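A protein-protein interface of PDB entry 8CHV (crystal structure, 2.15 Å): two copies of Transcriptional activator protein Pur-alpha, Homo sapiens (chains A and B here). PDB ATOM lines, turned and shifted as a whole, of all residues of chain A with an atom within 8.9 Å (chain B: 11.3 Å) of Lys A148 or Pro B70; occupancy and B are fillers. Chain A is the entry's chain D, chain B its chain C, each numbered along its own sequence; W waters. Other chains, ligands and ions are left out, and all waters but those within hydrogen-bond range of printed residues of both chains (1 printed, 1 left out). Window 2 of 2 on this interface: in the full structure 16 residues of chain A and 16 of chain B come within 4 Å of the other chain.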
ATOM      1  N   ALA A   6     -13.613 -13.369  19.032  1.00  0.00           N
ATOM      2  CA  ALA A   6     -13.286 -14.770  19.245  1.00  0.00           C
ATOM      3  C   ALA A   6     -14.138 -15.647  18.334  1.00  0.00           C
ATOM      4  O   ALA A   6     -15.232 -15.264  17.917  1.00  0.00           O
ATOM      5  CB  ALA A   6     -13.444 -15.142  20.709  1.00  0.00           C
ATOM      6  N   SER A   7     -13.602 -16.825  18.017  1.00  0.00           N
ATOM      7  CA  SER A   7     -14.358 -17.849  17.323  1.00  0.00           C
ATOM      8  C   SER A   7     -14.325 -19.133  18.146  1.00  0.00           C
ATOM      9  O   SER A   7     -13.455 -19.332  18.989  1.00  0.00           O
ATOM     10  CB  SER A   7     -13.846 -18.054  15.917  1.00  0.00           C
ATOM     11  OG  SER A   7     -14.308 -19.286  15.381  1.00  0.00           O
ATOM     12  N   LYS A   8     -15.316 -19.988  17.916  1.00  0.00           N
ATOM     13  CA  LYS A   8     -15.298 -21.342  18.428  1.00  0.00           C
ATOM     14  C   LYS A   8     -16.005 -22.226  17.412  1.00  0.00           C
ATOM     15  O   LYS A   8     -17.049 -21.841  16.894  1.00  0.00           O
ATOM     16  CB  LYS A   8     -15.976 -21.383  19.799  1.00  0.00           C
ATOM     17  CG  LYS A   8     -16.001 -22.756  20.449  1.00  0.00           C
ATOM     18  CD  LYS A   8     -14.633 -23.286  20.827  1.00  0.00           C
ATOM     19  CE  LYS A   8     -14.696 -24.670  21.438  1.00  0.00           C
ATOM     20  NZ  LYS A   8     -13.337 -25.185  21.740  1.00  0.00           N
ATOM     21  N   LEU A  19     -19.251 -20.512  16.068  1.00  0.00           N
ATOM     22  CA  LEU A  19     -19.714 -19.412  16.898  1.00  0.00           C
ATOM     23  C   LEU A  19     -18.631 -18.329  16.933  1.00  0.00           C
ATOM     24  O   LEU A  19     -17.536 -18.584  17.440  1.00  0.00           O
ATOM     25  CB  LEU A  19     -20.000 -19.946  18.310  1.00  0.00           C
ATOM     26  CG  LEU A  19     -21.006 -21.091  18.451  1.00  0.00           C
ATOM     27  CD1 LEU A  19     -20.406 -22.417  18.016  1.00  0.00           C
ATOM     28  CD2 LEU A  19     -21.482 -21.185  19.903  1.00  0.00           C
ATOM     29  N   VAL A  21     -17.761 -14.350  18.035  1.00  0.00           N
ATOM     30  CA  VAL A  21     -18.084 -13.100  18.716  1.00  0.00           C
ATOM     31  C   VAL A  21     -17.424 -11.947  17.955  1.00  0.00           C
ATOM     32  O   VAL A  21     -16.410 -12.134  17.286  1.00  0.00           O
ATOM     33  CB  VAL A  21     -17.746 -13.109  20.228  1.00  0.00           C
ATOM     34  CG1 VAL A  21     -16.321 -13.531  20.509  1.00  0.00           C
ATOM     35  CG2 VAL A  21     -18.030 -11.766  20.907  1.00  0.00           C
ATOM     36  N   LEU A  30     -23.029 -12.227  18.608  1.00  0.00           N
ATOM     37  CA  LEU A  30     -22.601 -13.520  18.085  1.00  0.00           C
ATOM     38  C   LEU A  30     -23.154 -13.737  16.687  1.00  0.00           C
ATOM     39  O   LEU A  30     -24.277 -13.336  16.400  1.00  0.00           O
ATOM     40  CB  LEU A  30     -23.092 -14.651  18.990  1.00  0.00           C
ATOM     41  CG  LEU A  30     -22.335 -14.845  20.299  1.00  0.00           C
ATOM     42  CD1 LEU A  30     -23.112 -15.781  21.206  1.00  0.00           C
ATOM     43  CD2 LEU A  30     -20.927 -15.379  20.049  1.00  0.00           C
ATOM     44  N   MET A  48     -25.640 -10.204  22.724  1.00  0.00           N
ATOM     45  CA  MET A  48     -25.123 -10.907  23.883  1.00  0.00           C
ATOM     46  C   MET A  48     -26.246 -11.158  24.881  1.00  0.00           C
ATOM     47  O   MET A  48     -26.411 -12.285  25.342  1.00  0.00           O
ATOM     48  CB  MET A  48     -23.996 -10.107  24.537  1.00  0.00           C
ATOM     49  CG  MET A  48     -22.667 -10.431  23.911  1.00  0.00           C
ATOM     50  SD  MET A  48     -22.169 -12.121  24.309  1.00  0.00           S
ATOM     51  CE  MET A  48     -20.995 -12.392  22.982  1.00  0.00           C
ATOM     52  N   ARG A  55     -28.852 -19.615  25.347  1.00  0.00           N
ATOM     53  CA  ARG A  55     -28.146 -20.599  26.144  1.00  0.00           C
ATOM     54  C   ARG A  55     -29.108 -21.314  27.096  1.00  0.00           C
ATOM     55  O   ARG A  55     -29.037 -22.535  27.262  1.00  0.00           O
ATOM     56  CB  ARG A  55     -27.041 -19.906  26.944  1.00  0.00           C
ATOM     57  CG  ARG A  55     -26.265 -20.828  27.875  1.00  0.00           C
ATOM     58  CD  ARG A  55     -25.713 -20.068  29.061  1.00  0.00           C
ATOM     59  NE  ARG A  55     -26.736 -19.452  29.909  1.00  0.00           N
ATOM     60  CZ  ARG A  55     -26.518 -18.401  30.696  1.00  0.00           C
ATOM     61  NH1 ARG A  55     -25.328 -17.819  30.705  1.00  0.00           N
ATOM     62  NH2 ARG A  55     -27.495 -17.916  31.449  1.00  0.00           N
ATOM     63  N   ILE A 140     -25.236 -30.408  23.758  1.00  0.00           N
ATOM     64  CA  ILE A 140     -24.473 -30.134  24.956  1.00  0.00           C
ATOM     65  C   ILE A 140     -23.163 -29.436  24.576  1.00  0.00           C
ATOM     66  O   ILE A 140     -22.794 -28.430  25.204  1.00  0.00           O
ATOM     67  CB  ILE A 140     -24.285 -31.401  25.798  1.00  0.00           C
ATOM     68  CG1 ILE A 140     -25.599 -31.783  26.478  1.00  0.00           C
ATOM     69  CG2 ILE A 140     -23.155 -31.216  26.798  1.00  0.00           C
ATOM     70  CD1 ILE A 140     -25.662 -33.210  26.938  1.00  0.00           C
ATOM     71  N   GLU A 141     -22.488 -29.936  23.531  1.00  0.00           N
ATOM     72  CA  GLU A 141     -21.277 -29.287  23.041  1.00  0.00           C
ATOM     73  C   GLU A 141     -21.582 -27.845  22.619  1.00  0.00           C
ATOM     74  O   GLU A 141     -20.938 -26.899  23.050  1.00  0.00           O
ATOM     75  CB  GLU A 141     -20.651 -30.061  21.878  1.00  0.00           C
ATOM     76  CG  GLU A 141     -19.936 -31.343  22.276  1.00  0.00           C
ATOM     77  CD  GLU A 141     -19.000 -31.311  23.477  1.00  0.00           C
ATOM     78  OE1 GLU A 141     -18.032 -30.537  23.431  1.00  0.00           O
ATOM     79  OE2 GLU A 141     -19.235 -32.075  24.455  1.00  0.00           O
ATOM     80  N   PHE A 142     -22.588 -27.672  21.777  1.00  0.00           N
ATOM     81  CA  PHE A 142     -22.928 -26.351  21.300  1.00  0.00           C
ATOM     82  C   PHE A 142     -23.170 -25.429  22.490  1.00  0.00           C
ATOM     83  O   PHE A 142     -22.565 -24.375  22.625  1.00  0.00           O
ATOM     84  CB  PHE A 142     -24.152 -26.451  20.390  1.00  0.00           C
ATOM     85  CG  PHE A 142     -24.468 -25.173  19.657  1.00  0.00           C
ATOM     86  CD1 PHE A 142     -23.832 -24.864  18.463  1.00  0.00           C
ATOM     87  CD2 PHE A 142     -25.372 -24.275  20.186  1.00  0.00           C
ATOM     88  CE1 PHE A 142     -24.115 -23.681  17.791  1.00  0.00           C
ATOM     89  CE2 PHE A 142     -25.654 -23.094  19.523  1.00  0.00           C
ATOM     90  CZ  PHE A 142     -25.030 -22.802  18.322  1.00  0.00           C
ATOM     91  N   ARG A 143     -24.066 -25.853  23.372  1.00  0.00           N
ATOM     92  CA  ARG A 143     -24.447 -25.053  24.525  1.00  0.00           C
ATOM     93  C   ARG A 143     -23.202 -24.647  25.292  1.00  0.00           C
ATOM     94  O   ARG A 143     -23.068 -23.492  25.670  1.00  0.00           O
ATOM     95  CB  ARG A 143     -25.420 -25.832  25.411  1.00  0.00           C
ATOM     96  CG  ARG A 143     -26.154 -24.975  26.427  1.00  0.00           C
ATOM     97  CD  ARG A 143     -25.313 -24.682  27.662  1.00  0.00           C
ATOM     98  NE  ARG A 143     -24.643 -25.874  28.141  1.00  0.00           N
ATOM     99  CZ  ARG A 143     -25.248 -26.783  28.896  1.00  0.00           C
ATOM    100  NH1 ARG A 143     -26.473 -26.528  29.338  1.00  0.00           N
ATOM    101  NH2 ARG A 143     -24.595 -27.876  29.273  1.00  0.00           N
ATOM    102  N   ASP A 144     -22.294 -25.606  25.500  1.00  0.00           N
ATOM    103  CA  ASP A 144     -21.076 -25.370  26.255  1.00  0.00           C
ATOM    104  C   ASP A 144     -20.176 -24.353  25.549  1.00  0.00           C
ATOM    105  O   ASP A 144     -19.680 -23.432  26.198  1.00  0.00           O
ATOM    106  CB  ASP A 144     -20.351 -26.687  26.551  1.00  0.00           C
ATOM    107  CG  ASP A 144     -20.996 -27.531  27.644  1.00  0.00           C
ATOM    108  OD1 ASP A 144     -22.016 -27.081  28.233  1.00  0.00           O
ATOM    109  OD2 ASP A 144     -20.511 -28.670  27.855  1.00  0.00           O
ATOM    110  N   ALA A 145     -19.975 -24.486  24.229  1.00  0.00           N
ATOM    111  CA  ALA A 145     -19.179 -23.526  23.478  1.00  0.00           C
ATOM    112  C   ALA A 145     -19.765 -22.121  23.618  1.00  0.00           C
ATOM    113  O   ALA A 145     -19.070 -21.144  23.877  1.00  0.00           O
ATOM    114  CB  ALA A 145     -19.125 -23.952  22.034  1.00  0.00           C
ATOM    115  N   LEU A 146     -21.082 -22.029  23.486  1.00  0.00           N
ATOM    116  CA  LEU A 146     -21.771 -20.759  23.607  1.00  0.00           C
ATOM    117  C   LEU A 146     -21.668 -20.212  25.023  1.00  0.00           C
ATOM    118  O   LEU A 146     -21.667 -19.000  25.200  1.00  0.00           O
ATOM    119  CB  LEU A 146     -23.235 -20.968  23.227  1.00  0.00           C
ATOM    120  CG  LEU A 146     -24.164 -19.795  23.515  1.00  0.00           C
ATOM    121  CD1 LEU A 146     -23.668 -18.535  22.825  1.00  0.00           C
ATOM    122  CD2 LEU A 146     -25.580 -20.111  23.065  1.00  0.00           C
ATOM    123  N   ALA A 147     -21.642 -21.084  26.038  1.00  0.00           N
ATOM    124  CA  ALA A 147     -21.666 -20.630  27.427  1.00  0.00           C
ATOM    125  C   ALA A 147     -20.336 -19.980  27.785  1.00  0.00           C
ATOM    126  O   ALA A 147     -20.303 -18.960  28.470  1.00  0.00           O
ATOM    127  CB  ALA A 147     -21.962 -21.773  28.354  1.00  0.00           C
ATOM    128  N   LYS A 148     -19.258 -20.585  27.283  1.00  0.00           N
ATOM    129  CA  LYS A 148     -17.898 -20.102  27.466  1.00  0.00           C
ATOM    130  C   LYS A 148     -17.783 -18.691  26.892  1.00  0.00           C
ATOM    131  O   LYS A 148     -17.292 -17.782  27.559  1.00  0.00           O
ATOM    132  CB  LYS A 148     -16.937 -21.093  26.797  1.00  0.00           C
ATOM    133  CG  LYS A 148     -15.467 -20.703  26.773  1.00  0.00           C
ATOM    134  CD  LYS A 148     -14.578 -21.768  26.139  1.00  0.00           C
ATOM    135  CE  LYS A 148     -13.282 -21.243  25.553  1.00  0.00           C
ATOM    136  NZ  LYS A 148     -12.458 -20.565  26.581  1.00  0.00           N
ATOM    137  N   LEU A 149     -18.234 -18.518  25.648  1.00  0.00           N
ATOM    138  CA  LEU A 149     -18.128 -17.231  24.985  1.00  0.00           C
ATOM    139  C   LEU A 149     -18.967 -16.190  25.719  1.00  0.00           C
ATOM    140  O   LEU A 149     -18.589 -15.022  25.752  1.00  0.00           O
ATOM    141  CB  LEU A 149     -18.598 -17.357  23.538  1.00  0.00           C
ATOM    142  CG  LEU A 149     -17.744 -18.183  22.576  1.00  0.00           C
ATOM    143  CD1 LEU A 149     -18.435 -18.265  21.199  1.00  0.00           C
ATOM    144  CD2 LEU A 149     -16.359 -17.595  22.408  1.00  0.00           C
ATOM    145  N   ILE A 150     -20.110 -16.594  26.281  1.00  0.00           N
ATOM    146  CA  ILE A 150     -20.912 -15.678  27.075  1.00  0.00           C
ATOM    147  C   ILE A 150     -20.202 -15.349  28.401  1.00  0.00           C
ATOM    148  O   ILE A 150     -20.276 -14.213  28.877  1.00  0.00           O
ATOM    149  CB  ILE A 150     -22.328 -16.234  27.331  1.00  0.00           C
ATOM    150  CG1 ILE A 150     -23.169 -16.354  26.061  1.00  0.00           C
ATOM    151  CG2 ILE A 150     -23.067 -15.405  28.371  1.00  0.00           C
ATOM    152  CD1 ILE A 150     -24.555 -16.937  26.301  1.00  0.00           C
ATOM    153  N   ASP A 151     -19.553 -16.330  29.048  1.00  0.00           N
ATOM    154  CA  ASP A 151     -18.937 -16.081  30.348  1.00  0.00           C
ATOM    155  C   ASP A 151     -17.810 -15.068  30.121  1.00  0.00           C
ATOM    156  O   ASP A 151     -17.656 -14.105  30.874  1.00  0.00           O
ATOM    157  CB  ASP A 151     -18.583 -17.401  31.064  1.00  0.00           C
ATOM    158  CG  ASP A 151     -17.110 -17.737  31.304  1.00  0.00           C
ATOM    159  OD1 ASP A 151     -16.455 -17.040  32.128  1.00  0.00           O
ATOM    160  OD2 ASP A 151     -16.644 -18.753  30.737  1.00  0.00           O
ATOM    161  N   ASP A 152     -17.099 -15.258  29.000  1.00  0.00           N
ATOM    162  CA  ASP A 152     -15.969 -14.437  28.600  1.00  0.00           C
ATOM    163  C   ASP A 152     -16.422 -13.023  28.227  1.00  0.00           C
ATOM    164  O   ASP A 152     -15.922 -12.049  28.793  1.00  0.00           O
ATOM    165  CB  ASP A 152     -15.214 -15.121  27.451  1.00  0.00           C
ATOM    166  CG  ASP A 152     -14.447 -16.362  27.878  1.00  0.00           C
ATOM    167  OD1 ASP A 152     -14.326 -16.584  29.102  1.00  0.00           O
ATOM    168  OD2 ASP A 152     -13.986 -17.109  26.993  1.00  0.00           O
ATOM    169  N   TYR A 153     -17.367 -12.918  27.282  1.00  0.00           N
ATOM    170  CA  TYR A 153     -17.463 -11.720  26.467  1.00  0.00           C
ATOM    171  C   TYR A 153     -18.690 -10.886  26.817  1.00  0.00           C
ATOM    172  O   TYR A 153     -19.168 -10.136  25.975  1.00  0.00           O
ATOM    173  CB  TYR A 153     -17.360 -12.071  24.977  1.00  0.00           C
ATOM    174  CG  TYR A 153     -15.951 -12.381  24.525  1.00  0.00           C
ATOM    175  CD1 TYR A 153     -14.995 -11.384  24.400  1.00  0.00           C
ATOM    176  CD2 TYR A 153     -15.550 -13.685  24.287  1.00  0.00           C
ATOM    177  CE1 TYR A 153     -13.695 -11.669  24.009  1.00  0.00           C
ATOM    178  CE2 TYR A 153     -14.256 -13.988  23.889  1.00  0.00           C
ATOM    179  CZ  TYR A 153     -13.324 -12.976  23.737  1.00  0.00           C
ATOM    180  OH  TYR A 153     -12.038 -13.311  23.355  1.00  0.00           O
ATOM    181  N   GLY A 154     -19.141 -10.909  28.070  1.00  0.00           N
ATOM    182  CA  GLY A 154     -19.825  -9.724  28.568  1.00  0.00           C
ATOM    183  C   GLY A 154     -20.649  -9.963  29.824  1.00  0.00           C
ATOM    184  O   GLY A 154     -21.857 -10.141  29.728  1.00  0.00           O
ATOM    185  N   VAL A 155     -19.982  -9.943  30.985  1.00  0.00           N
ATOM    186  CA  VAL A 155     -20.640  -9.964  32.288  1.00  0.00           C
ATOM    187  C   VAL A 155     -19.899  -8.975  33.189  1.00  0.00           C
ATOM    188  O   VAL A 155     -19.088  -8.189  32.703  1.00  0.00           O
ATOM    189  CB  VAL A 155     -20.709 -11.382  32.908  1.00  0.00           C
ATOM    190  CG1 VAL A 155     -21.289 -11.375  34.321  1.00  0.00           C
ATOM    191  CG2 VAL A 155     -21.468 -12.370  32.028  1.00  0.00           C
ATOM    192  N   HIS B  64     -24.586 -36.046  34.285  1.00  0.00           N
ATOM    193  CA  HIS B  64     -23.381 -35.392  34.769  1.00  0.00           C
ATOM    194  C   HIS B  64     -22.778 -34.571  33.630  1.00  0.00           C
ATOM    195  O   HIS B  64     -22.422 -33.415  33.842  1.00  0.00           O
ATOM    196  CB  HIS B  64     -22.455 -36.405  35.461  1.00  0.00           C
ATOM    197  CG  HIS B  64     -21.185 -35.841  36.032  1.00  0.00           C
ATOM    198  ND1 HIS B  64     -20.896 -35.820  37.384  1.00  0.00           N
ATOM    199  CD2 HIS B  64     -20.118 -35.285  35.419  1.00  0.00           C
ATOM    200  CE1 HIS B  64     -19.710 -35.251  37.569  1.00  0.00           C
ATOM    201  NE2 HIS B  64     -19.216 -34.921  36.386  1.00  0.00           N
ATOM    202  N   TYR B  65     -22.756 -35.149  32.419  1.00  0.00           N
ATOM    203  CA  TYR B  65     -22.259 -34.503  31.199  1.00  0.00           C
ATOM    204  C   TYR B  65     -23.067 -33.249  30.856  1.00  0.00           C
ATOM    205  O   TYR B  65     -22.478 -32.226  30.539  1.00  0.00           O
ATOM    206  CB  TYR B  65     -22.223 -35.521  30.056  1.00  0.00           C
ATOM    207  CG  TYR B  65     -21.979 -35.007  28.657  1.00  0.00           C
ATOM    208  CD1 TYR B  65     -20.905 -34.189  28.347  1.00  0.00           C
ATOM    209  CD2 TYR B  65     -22.810 -35.394  27.611  1.00  0.00           C
ATOM    210  CE1 TYR B  65     -20.683 -33.756  27.045  1.00  0.00           C
ATOM    211  CE2 TYR B  65     -22.597 -34.970  26.308  1.00  0.00           C
ATOM    212  CZ  TYR B  65     -21.537 -34.137  26.023  1.00  0.00           C
ATOM    213  OH  TYR B  65     -21.354 -33.734  24.729  1.00  0.00           O
ATOM    214  N   ALA B  66     -24.405 -33.307  30.917  1.00  0.00           N
ATOM    215  CA  ALA B  66     -25.218 -32.126  30.652  1.00  0.00           C
ATOM    216  C   ALA B  66     -24.937 -30.998  31.655  1.00  0.00           C
ATOM    217  O   ALA B  66     -25.118 -29.832  31.316  1.00  0.00           O
ATOM    218  CB  ALA B  66     -26.684 -32.489  30.653  1.00  0.00           C
ATOM    219  N   GLN B  67     -24.511 -31.344  32.885  1.00  0.00           N
ATOM    220  CA  GLN B  67     -24.303 -30.375  33.950  1.00  0.00           C
ATOM    221  C   GLN B  67     -22.852 -29.877  34.028  1.00  0.00           C
ATOM    222  O   GLN B  67     -22.584 -28.983  34.827  1.00  0.00           O
ATOM    223  CB  GLN B  67     -24.672 -30.970  35.317  1.00  0.00           C
ATOM    224  CG  GLN B  67     -26.170 -31.014  35.613  1.00  0.00           C
ATOM    225  CD  GLN B  67     -26.455 -31.328  37.065  1.00  0.00           C
ATOM    226  OE1 GLN B  67     -26.191 -30.523  37.959  1.00  0.00           O
ATOM    227  NE2 GLN B  67     -27.003 -32.510  37.315  1.00  0.00           N
ATOM    228  N   LEU B  68     -21.921 -30.431  33.232  1.00  0.00           N
ATOM    229  CA  LEU B  68     -20.519 -30.028  33.296  1.00  0.00           C
ATOM    230  C   LEU B  68     -20.348 -28.529  33.026  1.00  0.00           C
ATOM    231  O   LEU B  68     -19.609 -27.835  33.738  1.00  0.00           O
ATOM    232  CB  LEU B  68     -19.710 -30.820  32.264  1.00  0.00           C
ATOM    233  CG  LEU B  68     -19.336 -32.249  32.644  1.00  0.00           C
ATOM    234  CD1 LEU B  68     -18.507 -32.895  31.542  1.00  0.00           C
ATOM    235  CD2 LEU B  68     -18.589 -32.288  33.974  1.00  0.00           C
ATOM    236  N   GLY B  69     -21.020 -28.049  31.965  1.00  0.00           N
ATOM    237  CA  GLY B  69     -20.671 -26.792  31.334  1.00  0.00           C
ATOM    238  C   GLY B  69     -19.317 -26.900  30.633  1.00  0.00           C
ATOM    239  O   GLY B  69     -18.731 -27.984  30.542  1.00  0.00           O
ATOM    240  N   PRO B  70     -18.761 -25.775  30.131  1.00  0.00           N
ATOM    241  CA  PRO B  70     -17.448 -25.803  29.469  1.00  0.00           C
ATOM    242  C   PRO B  70     -16.307 -26.243  30.405  1.00  0.00           C
ATOM    243  O   PRO B  70     -16.416 -26.126  31.630  1.00  0.00           O
ATOM    244  CB  PRO B  70     -17.285 -24.359  28.947  1.00  0.00           C
ATOM    245  CG  PRO B  70     -18.229 -23.508  29.794  1.00  0.00           C
ATOM    246  CD  PRO B  70     -19.355 -24.429  30.209  1.00  0.00           C
ATOM    247  N   SER B  71     -15.227 -26.785  29.815  1.00  0.00           N
ATOM    248  CA  SER B  71     -14.067 -27.268  30.555  1.00  0.00           C
ATOM    249  C   SER B  71     -13.564 -26.208  31.548  1.00  0.00           C
ATOM    250  O   SER B  71     -12.663 -25.428  31.161  1.00  0.00           O
ATOM    251  CB  SER B  71     -12.957 -27.701  29.618  1.00  0.00           C
ATOM    252  OG  SER B  71     -13.222 -28.991  29.082  1.00  0.00           O
ATOM    253  N   LEU B  87     -13.944 -37.775  35.484  1.00  0.00           N
ATOM    254  CA  LEU B  87     -14.986 -36.861  35.923  1.00  0.00           C
ATOM    255  C   LEU B  87     -16.019 -37.631  36.734  1.00  0.00           C
ATOM    256  O   LEU B  87     -16.668 -37.062  37.597  1.00  0.00           O
ATOM    257  CB  LEU B  87     -15.630 -36.217  34.695  1.00  0.00           C
ATOM    258  CG  LEU B  87     -14.772 -35.186  33.967  1.00  0.00           C
ATOM    259  CD1 LEU B  87     -15.396 -34.828  32.623  1.00  0.00           C
ATOM    260  CD2 LEU B  87     -14.590 -33.938  34.822  1.00  0.00           C
ATOM    261  N   GLU B 105     -12.156 -36.842  29.940  1.00  0.00           N
ATOM    262  CA  GLU B 105     -12.006 -35.953  28.803  1.00  0.00           C
ATOM    263  C   GLU B 105     -10.543 -35.740  28.456  1.00  0.00           C
ATOM    264  O   GLU B 105      -9.671 -35.851  29.302  1.00  0.00           O
ATOM    265  CB  GLU B 105     -12.685 -34.602  29.030  1.00  0.00           C
ATOM    266  CG  GLU B 105     -12.137 -33.776  30.172  1.00  0.00           C
ATOM    267  CD  GLU B 105     -12.868 -32.451  30.316  1.00  0.00           C
ATOM    268  OE1 GLU B 105     -13.705 -32.106  29.420  1.00  0.00           O
ATOM    269  OE2 GLU B 105     -12.605 -31.767  31.325  1.00  0.00           O
ATOM    270  N   ASN B 106     -10.341 -35.367  27.193  1.00  0.00           N
ATOM    271  CA  ASN B 106      -9.043 -35.284  26.556  1.00  0.00           C
ATOM    272  C   ASN B 106      -9.142 -34.193  25.485  1.00  0.00           C
ATOM    273  O   ASN B 106     -10.219 -33.624  25.297  1.00  0.00           O
ATOM    274  CB  ASN B 106      -8.624 -36.661  26.024  1.00  0.00           C
ATOM    275  CG  ASN B 106      -9.335 -37.050  24.743  1.00  0.00           C
ATOM    276  OD1 ASN B 106      -8.696 -37.385  23.746  1.00  0.00           O
ATOM    277  ND2 ASN B 106     -10.658 -36.996  24.749  1.00  0.00           N
ATOM    278  N   GLY B 109     -12.145 -34.240  23.127  1.00  0.00           N
ATOM    279  CA  GLY B 109     -13.433 -34.056  23.782  1.00  0.00           C
ATOM    280  C   GLY B 109     -13.716 -35.111  24.853  1.00  0.00           C
ATOM    281  O   GLY B 109     -12.841 -35.913  25.170  1.00  0.00           O
ATOM    282  N   ARG B 110     -14.945 -35.083  25.396  1.00  0.00           N
ATOM    283  CA  ARG B 110     -15.372 -35.954  26.479  1.00  0.00           C
ATOM    284  C   ARG B 110     -15.773 -37.329  25.948  1.00  0.00           C
ATOM    285  O   ARG B 110     -16.264 -37.454  24.840  1.00  0.00           O
ATOM    286  CB  ARG B 110     -16.587 -35.387  27.219  1.00  0.00           C
ATOM    287  CG  ARG B 110     -16.303 -34.227  28.166  1.00  0.00           C
ATOM    288  CD  ARG B 110     -16.438 -32.839  27.552  1.00  0.00           C
ATOM    289  NE  ARG B 110     -16.720 -31.827  28.572  1.00  0.00           N
ATOM    290  CZ  ARG B 110     -17.714 -30.936  28.509  1.00  0.00           C
ATOM    291  NH1 ARG B 110     -18.454 -30.815  27.412  1.00  0.00           N
ATOM    292  NH2 ARG B 110     -17.931 -30.125  29.533  1.00  0.00           N
HETATM  293  O   HOH W   1     -23.316 -32.765  22.966  1.00  0.00           O
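The side-chain hydroxyl of Tyr B65 sits at hydrogen-bond distance from the side-chain carboxylate of Glu A141 (2.7 Å). The backbone carbonyl oxygen (O) of Ala B66 sits at hydrogen-bond distance from the guanidinium group (NH2) of Arg A143, at 2.9 Å. The guanidinium group (NH1) of Arg B110 is in salt-bridge range of the side-chain carboxylate (OE2) of Glu A141, 3.3 Å away. The guanidinium group (NH1) of Arg B110 lies within salt-bridge range of the side-chain carboxylate (OD2) of Asp A144 (3.0 Å). The side-chain carboxylate (OD2) of Asp A144 sits close to the backbone carbonyl oxygen (O) of Gly B69, at 3.3 Å.
The backbone carbonyl oxygen (O) of Gly B69 lies within hydrogen-bond range of the guanidinium group (NH2) of Arg B110 (2.5 Å). The guanidinium group (NE) of Arg B110 lies within salt-bridge range of the side-chain carboxylate (OE1) of Glu B105. The guanidinium group (NH2) of Arg A143 is in salt-bridge range of the side-chain carboxylate (OD1) of Asp A144, at 2.9 Å. NZ of Lys A148 is in salt-bridge range of OD2 of Asp A152, 3.8 Å away.
Among the printed residues, merely in contact across the chains: Ile A140 with Tyr B65, Asp A144 with Pro B70, Ile A140 with Ala B66 and Lys A148 with Pro B70.
Leu A19 touches none of the printed residues of chain B. Of the printed residues of chain B, Ile A140 touches Tyr B65 and Ala B66. Phe A142 touches none of the printed residues of chain B. Of the printed residues of chain B, Arg A143 touches Ala B66 (2.9 Å). No residue of chain B comes within 4 Å of Ala A145. No residue of chain B comes within 4 Å of Ala A147. Lys A148 touches one residue of chain B. No residue of chain B comes within 4 Å of Leu A149. No residue of chain B comes within 4 Å of Asp A152. Of the printed residues of chain A, Tyr B65 touches Ile A140 and Glu A141. Of the printed residues of chain A, Ala B66 touches Ile A140 and Arg A143. Of the printed residues of chain A, Gly B69 touches Asp A144. No residue of chain A comes within 4 Å of Ser B71. The nearest residue of chain B that does not touch Lys A148 is Ser B71 (6.3 Å). The nearest residue of chain A that does not touch Pro B70 is Ala A147 (4.2 Å). The nearest printed residue of chain A that does not touch Tyr B65 is Asp A144 (4.9 Å).
Of the 24 printed residues of chain A, 5 touch a printed residue of chain B. Hydrophobic or aromatic side chains of chain A that line the printed part of chain B: Ile A140. Printed residues of chain B that touch a printed residue of chain A: Tyr B65, Ala B66, Gly B69, Pro B70 and Arg B110. Hydrophobic or aromatic side chains of chain B within 4 Å of the printed part of chain A: Tyr B65, Ala B66 and Pro B70. Along chain B the printed residues that touch a printed residue of chain A span positions 65 to 110.
No position is printed for both chains. Of the 9 pairs that touch across the chains among the printed residues, none has its exchanged pair printed and touching as well.
Water W1 lies within hydrogen-bond range of the side-chain hydroxyl (OH) of Tyr B65 (2.8 Å), the backbone NH (N) of Glu A141 (3.0 Å) and the backbone NH (N) of Ile A140 (3.1 Å).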
